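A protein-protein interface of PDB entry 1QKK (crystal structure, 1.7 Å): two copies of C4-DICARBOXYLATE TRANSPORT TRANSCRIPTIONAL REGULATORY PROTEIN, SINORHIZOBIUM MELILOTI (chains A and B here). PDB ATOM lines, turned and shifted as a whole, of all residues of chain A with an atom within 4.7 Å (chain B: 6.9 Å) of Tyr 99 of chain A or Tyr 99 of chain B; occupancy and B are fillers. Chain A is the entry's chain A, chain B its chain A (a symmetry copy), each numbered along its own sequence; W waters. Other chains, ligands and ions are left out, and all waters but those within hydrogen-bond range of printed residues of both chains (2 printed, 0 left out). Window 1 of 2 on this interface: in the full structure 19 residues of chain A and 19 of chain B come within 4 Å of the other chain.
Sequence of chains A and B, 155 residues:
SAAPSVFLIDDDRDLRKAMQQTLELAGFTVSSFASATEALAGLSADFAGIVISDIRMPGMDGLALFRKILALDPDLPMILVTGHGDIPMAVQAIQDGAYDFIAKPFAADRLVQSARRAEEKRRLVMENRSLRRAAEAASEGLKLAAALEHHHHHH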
ATOM      1  N   PRO A  77       5.204  -9.361  10.609  1.00  0.00           N
ATOM      2  CA  PRO A  77       6.364 -10.255  10.705  1.00  0.00           C
ATOM      3  C   PRO A  77       6.833 -10.692  12.086  1.00  0.00           C
ATOM      4  O   PRO A  77       7.023  -9.867  12.975  1.00  0.00           O
ATOM      5  CB  PRO A  77       7.474  -9.485   9.978  1.00  0.00           C
ATOM      6  CG  PRO A  77       6.766  -8.408   9.208  1.00  0.00           C
ATOM      7  CD  PRO A  77       5.618  -8.044  10.096  1.00  0.00           C
ATOM      8  N   MET A  78       7.035 -11.999  12.235  1.00  0.00           N
ATOM      9  CA  MET A  78       7.545 -12.596  13.465  1.00  0.00           C
ATOM     10  C   MET A  78       8.860 -13.291  13.139  1.00  0.00           C
ATOM     11  O   MET A  78       8.911 -14.124  12.238  1.00  0.00           O
ATOM     12  CB  MET A  78       6.582 -13.659  14.015  1.00  0.00           C
ATOM     13  CG  MET A  78       7.275 -14.723  14.889  1.00  0.00           C
ATOM     14  SD  MET A  78       7.848 -14.069  16.495  1.00  0.00           S
ATOM     15  CE  MET A  78       6.411 -14.579  17.473  1.00  0.00           C
ATOM     16  N   ILE A  79       9.915 -12.943  13.865  1.00  0.00           N
ATOM     17  CA  ILE A  79      11.216 -13.581  13.690  1.00  0.00           C
ATOM     18  C   ILE A  79      11.419 -14.389  14.960  1.00  0.00           C
ATOM     19  O   ILE A  79      11.315 -13.852  16.061  1.00  0.00           O
ATOM     20  CB  ILE A  79      12.361 -12.551  13.570  1.00  0.00           C
ATOM     21  CG1 ILE A  79      12.192 -11.741  12.285  1.00  0.00           C
ATOM     22  CG2 ILE A  79      13.718 -13.269  13.551  1.00  0.00           C
ATOM     23  CD1 ILE A  79      13.204 -10.616  12.130  1.00  0.00           C
ATOM     24  N   ILE A  94       8.159 -21.259   9.754  1.00  0.00           N
ATOM     25  CA  ILE A  94       8.278 -20.373   8.596  1.00  0.00           C
ATOM     26  C   ILE A  94       7.364 -20.892   7.485  1.00  0.00           C
ATOM     27  O   ILE A  94       6.688 -20.114   6.813  1.00  0.00           O
ATOM     28  CB  ILE A  94       9.745 -20.295   8.106  1.00  0.00           C
ATOM     29  CG1 ILE A  94      10.601 -19.631   9.194  1.00  0.00           C
ATOM     30  CG2 ILE A  94       9.825 -19.510   6.788  1.00  0.00           C
ATOM     31  CD1 ILE A  94      12.104 -19.631   8.913  1.00  0.00           C
ATOM     32  N   GLY A  97       4.037 -19.704   8.104  1.00  0.00           N
ATOM     33  CA  GLY A  97       3.747 -18.279   8.045  1.00  0.00           C
ATOM     34  C   GLY A  97       4.697 -17.357   8.787  1.00  0.00           C
ATOM     35  O   GLY A  97       4.637 -16.137   8.607  1.00  0.00           O
ATOM     36  N   ALA A  98       5.558 -17.915   9.634  1.00  0.00           N
ATOM     37  CA  ALA A  98       6.516 -17.095  10.377  1.00  0.00           C
ATOM     38  C   ALA A  98       7.469 -16.447   9.369  1.00  0.00           C
ATOM     39  O   ALA A  98       7.740 -17.020   8.313  1.00  0.00           O
ATOM     40  CB  ALA A  98       7.288 -17.955  11.375  1.00  0.00           C
ATOM     41  N   TYR A  99       7.989 -15.265   9.689  1.00  0.00           N
ATOM     42  CA  TYR A  99       8.855 -14.570   8.742  1.00  0.00           C
ATOM     43  C   TYR A  99      10.249 -15.152   8.534  1.00  0.00           C
ATOM     44  O   TYR A  99      10.672 -15.363   7.398  1.00  0.00           O
ATOM     45  CB  TYR A  99       8.988 -13.091   9.116  1.00  0.00           C
ATOM     46  CG  TYR A  99       9.562 -12.272   7.981  1.00  0.00           C
ATOM     47  CD1 TYR A  99       8.813 -12.031   6.831  1.00  0.00           C
ATOM     48  CD2 TYR A  99      10.881 -11.816   8.016  1.00  0.00           C
ATOM     49  CE1 TYR A  99       9.363 -11.365   5.736  1.00  0.00           C
ATOM     50  CE2 TYR A  99      11.442 -11.148   6.926  1.00  0.00           C
ATOM     51  CZ  TYR A  99      10.678 -10.931   5.790  1.00  0.00           C
ATOM     52  OH  TYR A  99      11.230 -10.302   4.692  1.00  0.00           O
ATOM     53  N   ASP A 100      10.965 -15.404   9.622  1.00  0.00           N
ATOM     54  CA  ASP A 100      12.314 -15.941   9.522  1.00  0.00           C
ATOM     55  C   ASP A 100      12.720 -16.382  10.913  1.00  0.00           C
ATOM     56  O   ASP A 100      11.935 -16.280  11.852  1.00  0.00           O
ATOM     57  CB  ASP A 100      13.270 -14.844   9.038  1.00  0.00           C
ATOM     58  CG  ASP A 100      14.527 -15.394   8.389  1.00  0.00           C
ATOM     59  OD1 ASP A 100      14.797 -16.609   8.499  1.00  0.00           O
ATOM     60  OD2 ASP A 100      15.256 -14.590   7.768  1.00  0.00           O
ATOM     61  N   ARG A 117      15.116  -6.794   7.253  1.00  0.00           N
ATOM     62  CA  ARG A 117      14.324  -7.386   6.179  1.00  0.00           C
ATOM     63  C   ARG A 117      12.862  -7.449   6.603  1.00  0.00           C
ATOM     64  O   ARG A 117      11.965  -7.175   5.805  1.00  0.00           O
ATOM     65  CB  ARG A 117      14.803  -8.805   5.830  1.00  0.00           C
ATOM     66  CG  ARG A 117      15.860  -8.870   4.733  1.00  0.00           C
ATOM     67  CD  ARG A 117      16.163 -10.324   4.344  1.00  0.00           C
ATOM     68  NE  ARG A 117      16.750 -11.065   5.455  1.00  0.00           N
ATOM     69  CZ  ARG A 117      18.051 -11.125   5.710  1.00  0.00           C
ATOM     70  NH1 ARG A 117      18.918 -10.494   4.925  1.00  0.00           N
ATOM     71  NH2 ARG A 117      18.483 -11.807   6.759  1.00  0.00           N
ATOM     72  N   ALA A 118      12.627  -7.812   7.864  1.00  0.00           N
ATOM     73  CA  ALA A 118      11.270  -7.913   8.393  1.00  0.00           C
ATOM     74  C   ALA A 118      10.604  -6.544   8.472  1.00  0.00           C
ATOM     75  O   ALA A 118       9.417  -6.403   8.164  1.00  0.00           O
ATOM     76  CB  ALA A 118      11.290  -8.561   9.775  1.00  0.00           C
ATOM     77  N   GLU A 120      11.283  -4.054   6.632  1.00  0.00           N
ATOM     78  CA  GLU A 120      11.035  -3.665   5.247  1.00  0.00           C
ATOM     79  C   GLU A 120       9.707  -4.244   4.776  1.00  0.00           C
ATOM     80  O   GLU A 120       8.909  -3.543   4.151  1.00  0.00           O
ATOM     81  CB  GLU A 120      12.167  -4.158   4.347  1.00  0.00           C
ATOM     82  CG  GLU A 120      11.958  -3.858   2.872  1.00  0.00           C
ATOM     83  CD  GLU A 120      13.160  -4.256   2.041  1.00  0.00           C
ATOM     84  OE1 GLU A 120      13.597  -5.417   2.161  1.00  0.00           O
ATOM     85  OE2 GLU A 120      13.667  -3.410   1.274  1.00  0.00           O
ATOM     86  N   LYS A 121       9.461  -5.521   5.059  1.00  0.00           N
ATOM     87  CA  LYS A 121       8.187  -6.105   4.651  1.00  0.00           C
ATOM     88  C   LYS A 121       7.035  -5.349   5.310  1.00  0.00           C
ATOM     89  O   LYS A 121       6.061  -4.977   4.649  1.00  0.00           O
ATOM     90  CB  LYS A 121       8.067  -7.580   5.049  1.00  0.00           C
ATOM     91  CG  LYS A 121       6.627  -8.073   4.876  1.00  0.00           C
ATOM     92  CD  LYS A 121       6.380  -9.506   5.287  1.00  0.00           C
ATOM     93  CE  LYS A 121       4.889  -9.820   5.129  1.00  0.00           C
ATOM     94  NZ  LYS A 121       4.554 -11.241   5.418  1.00  0.00           N
ATOM     95  N   VAL B  51      16.553 -12.309  -8.274  1.00  0.00           N
ATOM     96  CA  VAL B  51      17.773 -12.878  -8.815  1.00  0.00           C
ATOM     97  C   VAL B  51      18.475 -13.692  -7.736  1.00  0.00           C
ATOM     98  O   VAL B  51      18.569 -13.258  -6.587  1.00  0.00           O
ATOM     99  CB  VAL B  51      18.740 -11.778  -9.306  1.00  0.00           C
ATOM    100  CG1 VAL B  51      20.046 -12.399  -9.793  1.00  0.00           C
ATOM    101  CG2 VAL B  51      18.088 -10.988 -10.417  1.00  0.00           C
ATOM    102  N   PHE B  66      25.674  -7.892  -8.667  1.00  0.00           N
ATOM    103  CA  PHE B  66      24.908  -7.188  -7.643  1.00  0.00           C
ATOM    104  C   PHE B  66      24.999  -5.675  -7.836  1.00  0.00           C
ATOM    105  O   PHE B  66      23.982  -4.980  -7.845  1.00  0.00           O
ATOM    106  CB  PHE B  66      25.415  -7.559  -6.243  1.00  0.00           C
ATOM    107  CG  PHE B  66      24.995  -6.585  -5.172  1.00  0.00           C
ATOM    108  CD1 PHE B  66      23.648  -6.323  -4.941  1.00  0.00           C
ATOM    109  CD2 PHE B  66      25.950  -5.897  -4.431  1.00  0.00           C
ATOM    110  CE1 PHE B  66      23.256  -5.382  -3.989  1.00  0.00           C
ATOM    111  CE2 PHE B  66      25.569  -4.953  -3.475  1.00  0.00           C
ATOM    112  CZ  PHE B  66      24.222  -4.696  -3.256  1.00  0.00           C
ATOM    113  N   LEU B  76      15.195  -4.525  -6.585  1.00  0.00           N
ATOM    114  CA  LEU B  76      15.107  -5.781  -7.328  1.00  0.00           C
ATOM    115  C   LEU B  76      16.008  -6.673  -6.464  1.00  0.00           C
ATOM    116  O   LEU B  76      17.229  -6.572  -6.533  1.00  0.00           O
ATOM    117  CB  LEU B  76      15.698  -5.602  -8.731  1.00  0.00           C
ATOM    118  CG  LEU B  76      15.414  -6.700  -9.758  1.00  0.00           C
ATOM    119  CD1 LEU B  76      15.942  -6.260 -11.115  1.00  0.00           C
ATOM    120  CD2 LEU B  76      16.053  -8.003  -9.326  1.00  0.00           C
ATOM    121  N   PRO B  77      15.410  -7.558  -5.644  1.00  0.00           N
ATOM    122  CA  PRO B  77      16.148  -8.455  -4.747  1.00  0.00           C
ATOM    123  C   PRO B  77      17.160  -9.417  -5.353  1.00  0.00           C
ATOM    124  O   PRO B  77      16.857 -10.134  -6.301  1.00  0.00           O
ATOM    125  CB  PRO B  77      15.040  -9.228  -4.018  1.00  0.00           C
ATOM    126  CG  PRO B  77      13.783  -8.450  -4.277  1.00  0.00           C
ATOM    127  CD  PRO B  77      13.982  -7.918  -5.662  1.00  0.00           C
ATOM    128  N   MET B  78      18.357  -9.429  -4.770  1.00  0.00           N
ATOM    129  CA  MET B  78      19.434 -10.329  -5.169  1.00  0.00           C
ATOM    130  C   MET B  78      19.783 -11.204  -3.973  1.00  0.00           C
ATOM    131  O   MET B  78      20.069 -10.690  -2.895  1.00  0.00           O
ATOM    132  CB  MET B  78      20.699  -9.552  -5.561  1.00  0.00           C
ATOM    133  CG  MET B  78      21.998 -10.366  -5.394  1.00  0.00           C
ATOM    134  SD  MET B  78      22.160 -11.715  -6.614  1.00  0.00           S
ATOM    135  CE  MET B  78      23.187 -10.817  -7.807  1.00  0.00           C
ATOM    136  N   ILE B  79      19.751 -12.517  -4.164  1.00  0.00           N
ATOM    137  CA  ILE B  79      20.123 -13.459  -3.113  1.00  0.00           C
ATOM    138  C   ILE B  79      21.427 -14.071  -3.595  1.00  0.00           C
ATOM    139  O   ILE B  79      21.499 -14.578  -4.713  1.00  0.00           O
ATOM    140  CB  ILE B  79      19.080 -14.585  -2.940  1.00  0.00           C
ATOM    141  CG1 ILE B  79      17.766 -13.995  -2.431  1.00  0.00           C
ATOM    142  CG2 ILE B  79      19.595 -15.632  -1.942  1.00  0.00           C
ATOM    143  CD1 ILE B  79      16.633 -15.006  -2.340  1.00  0.00           C
ATOM    144  N   LEU B  80      22.454 -14.002  -2.758  1.00  0.00           N
ATOM    145  CA  LEU B  80      23.758 -14.548  -3.096  1.00  0.00           C
ATOM    146  C   LEU B  80      23.935 -15.955  -2.543  1.00  0.00           C
ATOM    147  O   LEU B  80      23.650 -16.199  -1.371  1.00  0.00           O
ATOM    148  CB  LEU B  80      24.864 -13.653  -2.535  1.00  0.00           C
ATOM    149  CG  LEU B  80      25.050 -12.287  -3.191  1.00  0.00           C
ATOM    150  CD1 LEU B  80      25.928 -11.398  -2.324  1.00  0.00           C
ATOM    151  CD2 LEU B  80      25.683 -12.484  -4.566  1.00  0.00           C
ATOM    152  N   ALA B  93      27.898  -7.587   1.537  1.00  0.00           N
ATOM    153  CA  ALA B  93      27.057  -7.276   0.385  1.00  0.00           C
ATOM    154  C   ALA B  93      25.643  -6.921   0.845  1.00  0.00           C
ATOM    155  O   ALA B  93      25.016  -6.017   0.295  1.00  0.00           O
ATOM    156  CB  ALA B  93      27.013  -8.461  -0.577  1.00  0.00           C
ATOM    157  N   ILE B  94      25.147  -7.635   1.852  1.00  0.00           N
ATOM    158  CA  ILE B  94      23.805  -7.368   2.370  1.00  0.00           C
ATOM    159  C   ILE B  94      23.790  -5.973   2.995  1.00  0.00           C
ATOM    160  O   ILE B  94      22.838  -5.214   2.815  1.00  0.00           O
ATOM    161  CB  ILE B  94      23.390  -8.438   3.409  1.00  0.00           C
ATOM    162  CG1 ILE B  94      23.272  -9.798   2.708  1.00  0.00           C
ATOM    163  CG2 ILE B  94      22.061  -8.045   4.075  1.00  0.00           C
ATOM    164  CD1 ILE B  94      23.022 -10.981   3.644  1.00  0.00           C
ATOM    165  N   GLY B  97      23.306  -3.564   0.381  1.00  0.00           N
ATOM    166  CA  GLY B  97      22.057  -3.537  -0.365  1.00  0.00           C
ATOM    167  C   GLY B  97      21.540  -4.868  -0.880  1.00  0.00           C
ATOM    168  O   GLY B  97      20.393  -4.949  -1.331  1.00  0.00           O
ATOM    169  N   ALA B  98      22.370  -5.906  -0.842  1.00  0.00           N
ATOM    170  CA  ALA B  98      21.942  -7.225  -1.308  1.00  0.00           C
ATOM    171  C   ALA B  98      20.817  -7.711  -0.390  1.00  0.00           C
ATOM    172  O   ALA B  98      20.786  -7.364   0.791  1.00  0.00           O
ATOM    173  CB  ALA B  98      23.116  -8.202  -1.288  1.00  0.00           C
ATOM    174  N   TYR B  99      19.902  -8.520  -0.917  1.00  0.00           N
ATOM    175  CA  TYR B  99      18.773  -8.967  -0.107  1.00  0.00           C
ATOM    176  C   TYR B  99      19.073  -9.984   0.987  1.00  0.00           C
ATOM    177  O   TYR B  99      18.676  -9.797   2.137  1.00  0.00           O
ATOM    178  CB  TYR B  99      17.653  -9.515  -0.998  1.00  0.00           C
ATOM    179  CG  TYR B  99      16.347  -9.643  -0.246  1.00  0.00           C
ATOM    180  CD1 TYR B  99      15.637  -8.508   0.142  1.00  0.00           C
ATOM    181  CD2 TYR B  99      15.866 -10.890   0.158  1.00  0.00           C
ATOM    182  CE1 TYR B  99      14.486  -8.606   0.921  1.00  0.00           C
ATOM    183  CE2 TYR B  99      14.714 -11.001   0.938  1.00  0.00           C
ATOM    184  CZ  TYR B  99      14.033  -9.855   1.319  1.00  0.00           C
ATOM    185  OH  TYR B  99      12.912  -9.946   2.118  1.00  0.00           O
ATOM    186  N   ASP B 100      19.765 -11.061   0.636  1.00  0.00           N
ATOM    187  CA  ASP B 100      20.083 -12.096   1.609  1.00  0.00           C
ATOM    188  C   ASP B 100      21.109 -13.006   0.966  1.00  0.00           C
ATOM    189  O   ASP B 100      21.534 -12.768  -0.161  1.00  0.00           O
ATOM    190  CB  ASP B 100      18.820 -12.903   1.931  1.00  0.00           C
ATOM    191  CG  ASP B 100      18.890 -13.606   3.275  1.00  0.00           C
ATOM    192  OD1 ASP B 100      19.982 -13.676   3.878  1.00  0.00           O
ATOM    193  OD2 ASP B 100      17.833 -14.100   3.725  1.00  0.00           O
ATOM    194  N   PHE B 101      21.514 -14.041   1.690  1.00  0.00           N
ATOM    195  CA  PHE B 101      22.465 -14.996   1.155  1.00  0.00           C
ATOM    196  C   PHE B 101      22.106 -16.384   1.654  1.00  0.00           C
ATOM    197  O   PHE B 101      21.442 -16.537   2.681  1.00  0.00           O
ATOM    198  CB  PHE B 101      23.908 -14.630   1.557  1.00  0.00           C
ATOM    199  CG  PHE B 101      24.288 -15.037   2.958  1.00  0.00           C
ATOM    200  CD1 PHE B 101      24.666 -16.346   3.239  1.00  0.00           C
ATOM    201  CD2 PHE B 101      24.265 -14.113   3.994  1.00  0.00           C
ATOM    202  CE1 PHE B 101      25.011 -16.730   4.528  1.00  0.00           C
ATOM    203  CE2 PHE B 101      24.611 -14.489   5.293  1.00  0.00           C
ATOM    204  CZ  PHE B 101      24.984 -15.799   5.558  1.00  0.00           C
ATOM    205  N   GLN B 113      12.460 -21.046   1.105  1.00  0.00           N
ATOM    206  CA  GLN B 113      12.031 -20.016   2.045  1.00  0.00           C
ATOM    207  C   GLN B 113      12.741 -18.695   1.784  1.00  0.00           C
ATOM    208  O   GLN B 113      12.154 -17.624   1.939  1.00  0.00           O
ATOM    209  CB  GLN B 113      12.266 -20.469   3.491  1.00  0.00           C
ATOM    210  CG  GLN B 113      11.414 -21.677   3.876  1.00  0.00           C
ATOM    211  CD  GLN B 113      11.558 -22.077   5.338  1.00  0.00           C
ATOM    212  OE1 GLN B 113      12.530 -21.714   6.003  1.00  0.00           O
ATOM    213  NE2 GLN B 113      10.592 -22.847   5.837  1.00  0.00           N
ATOM    214  N   SER B 114      14.008 -18.767   1.389  1.00  0.00           N
ATOM    215  CA  SER B 114      14.761 -17.552   1.113  1.00  0.00           C
ATOM    216  C   SER B 114      14.198 -16.871  -0.133  1.00  0.00           C
ATOM    217  O   SER B 114      13.989 -15.653  -0.149  1.00  0.00           O
ATOM    218  CB  SER B 114      16.242 -17.880   0.900  1.00  0.00           C
ATOM    219  OG  SER B 114      16.990 -16.697   0.702  1.00  0.00           O
ATOM    220  N   ALA B 115      13.953 -17.662  -1.171  1.00  0.00           N
ATOM    221  CA  ALA B 115      13.414 -17.130  -2.419  1.00  0.00           C
ATOM    222  C   ALA B 115      12.028 -16.537  -2.202  1.00  0.00           C
ATOM    223  O   ALA B 115      11.699 -15.486  -2.759  1.00  0.00           O
ATOM    224  CB  ALA B 115      13.351 -18.221  -3.469  1.00  0.00           C
ATOM    225  N   ARG B 116      11.211 -17.203  -1.394  1.00  0.00           N
ATOM    226  CA  ARG B 116       9.868 -16.699  -1.140  1.00  0.00           C
ATOM    227  C   ARG B 116       9.854 -15.353  -0.429  1.00  0.00           C
ATOM    228  O   ARG B 116       8.993 -14.515  -0.720  1.00  0.00           O
ATOM    229  CB  ARG B 116       9.046 -17.741  -0.378  1.00  0.00           C
ATOM    230  CG  ARG B 116       8.616 -18.860  -1.303  1.00  0.00           C
ATOM    231  CD  ARG B 116       7.801 -19.921  -0.617  1.00  0.00           C
ATOM    232  NE  ARG B 116       7.228 -20.827  -1.607  1.00  0.00           N
ATOM    233  CZ  ARG B 116       6.731 -22.022  -1.321  1.00  0.00           C
ATOM    234  NH1 ARG B 116       6.739 -22.458  -0.070  1.00  0.00           N
ATOM    235  NH2 ARG B 116       6.224 -22.777  -2.286  1.00  0.00           N
ATOM    236  N   ARG B 117      10.797 -15.125   0.484  1.00  0.00           N
ATOM    237  CA  ARG B 117      10.854 -13.840   1.174  1.00  0.00           C
ATOM    238  C   ARG B 117      11.224 -12.747   0.179  1.00  0.00           C
ATOM    239  O   ARG B 117      10.668 -11.649   0.216  1.00  0.00           O
ATOM    240  CB  ARG B 117      11.886 -13.846   2.313  1.00  0.00           C
ATOM    241  CG  ARG B 117      11.333 -14.256   3.674  1.00  0.00           C
ATOM    242  CD  ARG B 117      12.389 -14.085   4.774  1.00  0.00           C
ATOM    243  NE  ARG B 117      13.528 -14.973   4.567  1.00  0.00           N
ATOM    244  CZ  ARG B 117      13.605 -16.213   5.033  1.00  0.00           C
ATOM    245  NH1 ARG B 117      12.610 -16.722   5.750  1.00  0.00           N
ATOM    246  NH2 ARG B 117      14.675 -16.947   4.769  1.00  0.00           N
ATOM    247  N   ALA B 118      12.169 -13.053  -0.711  1.00  0.00           N
ATOM    248  CA  ALA B 118      12.616 -12.092  -1.716  1.00  0.00           C
ATOM    249  C   ALA B 118      11.510 -11.791  -2.722  1.00  0.00           C
ATOM    250  O   ALA B 118      11.329 -10.641  -3.131  1.00  0.00           O
ATOM    251  CB  ALA B 118      13.848 -12.626  -2.444  1.00  0.00           C
ATOM    252  N   GLU B 119      10.782 -12.826  -3.131  1.00  0.00           N
ATOM    253  CA  GLU B 119       9.689 -12.658  -4.088  1.00  0.00           C
ATOM    254  C   GLU B 119       8.616 -11.785  -3.450  1.00  0.00           C
ATOM    255  O   GLU B 119       8.004 -10.942  -4.114  1.00  0.00           O
ATOM    256  CB  GLU B 119       9.104 -14.026  -4.472  1.00  0.00           C
ATOM    257  CG  GLU B 119       7.951 -13.974  -5.483  1.00  0.00           C
ATOM    258  CD  GLU B 119       6.598 -13.685  -4.849  1.00  0.00           C
ATOM    259  OE1 GLU B 119       5.609 -13.496  -5.595  1.00  0.00           O
ATOM    260  OE2 GLU B 119       6.513 -13.655  -3.604  1.00  0.00           O
ATOM    261  N   GLU B 120       8.398 -11.985  -2.155  1.00  0.00           N
ATOM    262  CA  GLU B 120       7.407 -11.206  -1.418  1.00  0.00           C
ATOM    263  C   GLU B 120       7.785  -9.730  -1.444  1.00  0.00           C
ATOM    264  O   GLU B 120       6.932  -8.873  -1.682  1.00  0.00           O
ATOM    265  CB  GLU B 120       7.316 -11.695   0.026  1.00  0.00           C
ATOM    266  CG  GLU B 120       6.357 -10.892   0.890  1.00  0.00           C
ATOM    267  CD  GLU B 120       6.212 -11.491   2.274  1.00  0.00           C
ATOM    268  OE1 GLU B 120       7.249 -11.722   2.926  1.00  0.00           O
ATOM    269  OE2 GLU B 120       5.064 -11.733   2.705  1.00  0.00           O
ATOM    270  N   LYS B 121       9.054  -9.418  -1.192  1.00  0.00           N
ATOM    271  CA  LYS B 121       9.463  -8.018  -1.237  1.00  0.00           C
ATOM    272  C   LYS B 121       9.210  -7.448  -2.632  1.00  0.00           C
ATOM    273  O   LYS B 121       8.640  -6.363  -2.778  1.00  0.00           O
ATOM    274  CB  LYS B 121      10.951  -7.833  -0.919  1.00  0.00           C
ATOM    275  CG  LYS B 121      11.407  -6.411  -1.261  1.00  0.00           C
ATOM    276  CD  LYS B 121      12.873  -6.130  -1.034  1.00  0.00           C
ATOM    277  CE  LYS B 121      13.184  -4.701  -1.493  1.00  0.00           C
ATOM    278  NZ  LYS B 121      14.588  -4.289  -1.223  1.00  0.00           N
ATOM    279  N   ARG B 122       9.632  -8.172  -3.663  1.00  0.00           N
ATOM    280  CA  ARG B 122       9.446  -7.662  -5.017  1.00  0.00           C
ATOM    281  C   ARG B 122       7.970  -7.485  -5.354  1.00  0.00           C
ATOM    282  O   ARG B 122       7.594  -6.491  -5.973  1.00  0.00           O
ATOM    283  CB  ARG B 122      10.115  -8.574  -6.044  1.00  0.00           C
ATOM    284  CG  ARG B 122      10.189  -7.971  -7.451  1.00  0.00           C
ATOM    285  CD  ARG B 122      10.910  -6.621  -7.452  1.00  0.00           C
ATOM    286  NE  ARG B 122      11.202  -6.159  -8.809  1.00  0.00           N
ATOM    287  CZ  ARG B 122      11.751  -4.982  -9.099  1.00  0.00           C
ATOM    288  NH1 ARG B 122      12.070  -4.137  -8.131  1.00  0.00           N
ATOM    289  NH2 ARG B 122      11.985  -4.653 -10.361  1.00  0.00           N
HETATM  290  O   HOH W   1      11.985  -7.540   3.070  1.00  0.00           O
HETATM  291  O   HOH W   2       9.662 -10.354   2.435  1.00  0.00           O
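Water W2 lies within hydrogen-bond range of the side-chain hydroxyl of Tyr 99 of chain A (2.7 Å), the backbone carbonyl oxygen of Arg 117 of chain B (2.8 Å), the side-chain carboxylate of Glu 120 of chain B (2.8 Å) and the side-chain hydroxyl of Tyr 99 of chain B (3.3 Å). Water W1 lies within hydrogen-bond range of OH of Tyr 99 of chain B (2.7 Å), O of Arg 117 of chain A (2.8 Å), OE1 of Glu 120 of chain A (2.8 Å) and OH of Tyr 99 of chain A (3.3 Å).
Among the printed residues, pairs that only touch across the chains: Ile 94 of chain A with Gln 113 of chain B (3.4 Å), Tyr 99 of chain A with Glu 120 of chain B (3.5 Å) and Glu 120 of chain A with Tyr 99 of chain B (3.5 Å).
Tyr 99 of chain B touches its own counterpart, Tyr 99 of chain A. Tyr 99 of chain A touches Arg 117 of chain B, and with the chains exchanged Arg 117 of chain A touches Tyr 99 of chain B. Asp 100 of chain A touches Arg 117 of chain B, and with the chains exchanged Arg 117 of chain A touches Asp 100 of chain B. Of the 10 pairs that touch across the chains among the printed residues, 9 have their exchanged pair printed and touching as well.
Printed residues of chain B that touch a printed residue of chain A: Tyr 99, Asp 100, Gln 113, Arg 117, Glu 120 and Lys 121. Hydrophobic or aromatic side chains of chain A within 4 Å of the printed part of chain B: Ile 94 and Tyr 99. Among the printed residues, 10 pairs touch across the chains. Among the printed residues, Asp or Glu carboxylates within 4 Å of a Lys or Arg side-chain nitrogen of the other chain: Asp 100 of chain A with Arg 117 of chain B (3.5 Å), Arg 117 of chain A with Asp 100 of chain B (3.5 Å), Glu 120 of chain A with Lys 121 of chain B (2.8 Å) and Lys 121 of chain A with Glu 120 of chain B (2.8 Å).
Of the printed residues of chain B, Ile 94 of chain A touches Gln 113 (3.4 Å). Of chain B, only Tyr 99 (3.1 Å), Arg 117 (2.9 Å) and Glu 120 (3.5 Å) come within 4 Å of Tyr 99 of chain A. Of the printed residues of chain B, Asp 100 of chain A touches Arg 117. Val 51 of chain B touches none of the printed residues of chain A. Of chain A, only Tyr 99, Arg 117 and Glu 120 come within 4 Å of Tyr 99 of chain B. Phe 101 of chain B touches none of the printed residues of chain A. Of the printed residues of chain A, Arg 117 of chain B touches Tyr 99 (2.9 Å) and Asp 100 (3.5 Å). The nearest printed residue of chain A that does not touch Tyr 99 of chain B is Ala 118 of chain A (6.1 Å). The nearest printed residue of chain A that does not touch Asp 100 of chain B is Asp 100 of chain A (4.8 Å).
The side-chain hydroxyl (OH) of Tyr 99 of chain B is in hydrogen-bond range of the side-chain hydroxyl (OH) of Tyr 99 of chain A, at 3.1 Å. O of Tyr 99 of chain B sits at hydrogen-bond distance from NH1 of Arg 117 of chain A (2.9 Å). The guanidinium group (NH1) of Arg 117 of chain A lies within salt-bridge range of the side-chain carboxylate (OD1) of Asp 100 of chain B (3.5 Å). The side-chain carboxylate (OE2) of Glu 120 of chain B lies within salt-bridge range of the side-chain amino group (NZ) of Lys 121 of chain A, at 2.8 Å. The backbone carbonyl oxygen (O) of Tyr 99 of chain A is in hydrogen-bond range of the guanidinium group (NH1) of Arg 117 of chain B (2.9 Å). OE2 of Glu 120 of chain A lies within salt-bridge range of NZ of Lys 121 of chain B (2.8 Å). OD1 of Asp 100 of chain A lies within salt-bridge range of NH1 of Arg 117 of chain B, at 3.5 Å.
O of Met 78 of chain A lies within hydrogen-bond range of N of Tyr 99 of chain A (2.9 Å). The backbone carbonyl oxygen (O) of Met 78 of chain B is in hydrogen-bond range of the backbone NH (N) of Tyr 99 of chain B (2.9 Å). OH of Tyr 99 of chain A lies within hydrogen-bond range of O of Arg 117 of chain A (3.4 Å). O of Asp 100 of chain B sits at hydrogen-bond distance from N of Leu 80 of chain B. The side-chain hydroxyl (OH) of Tyr 99 of chain B sits at hydrogen-bond distance from the backbone carbonyl oxygen (O) of Arg 117 of chain B (3.4 Å).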
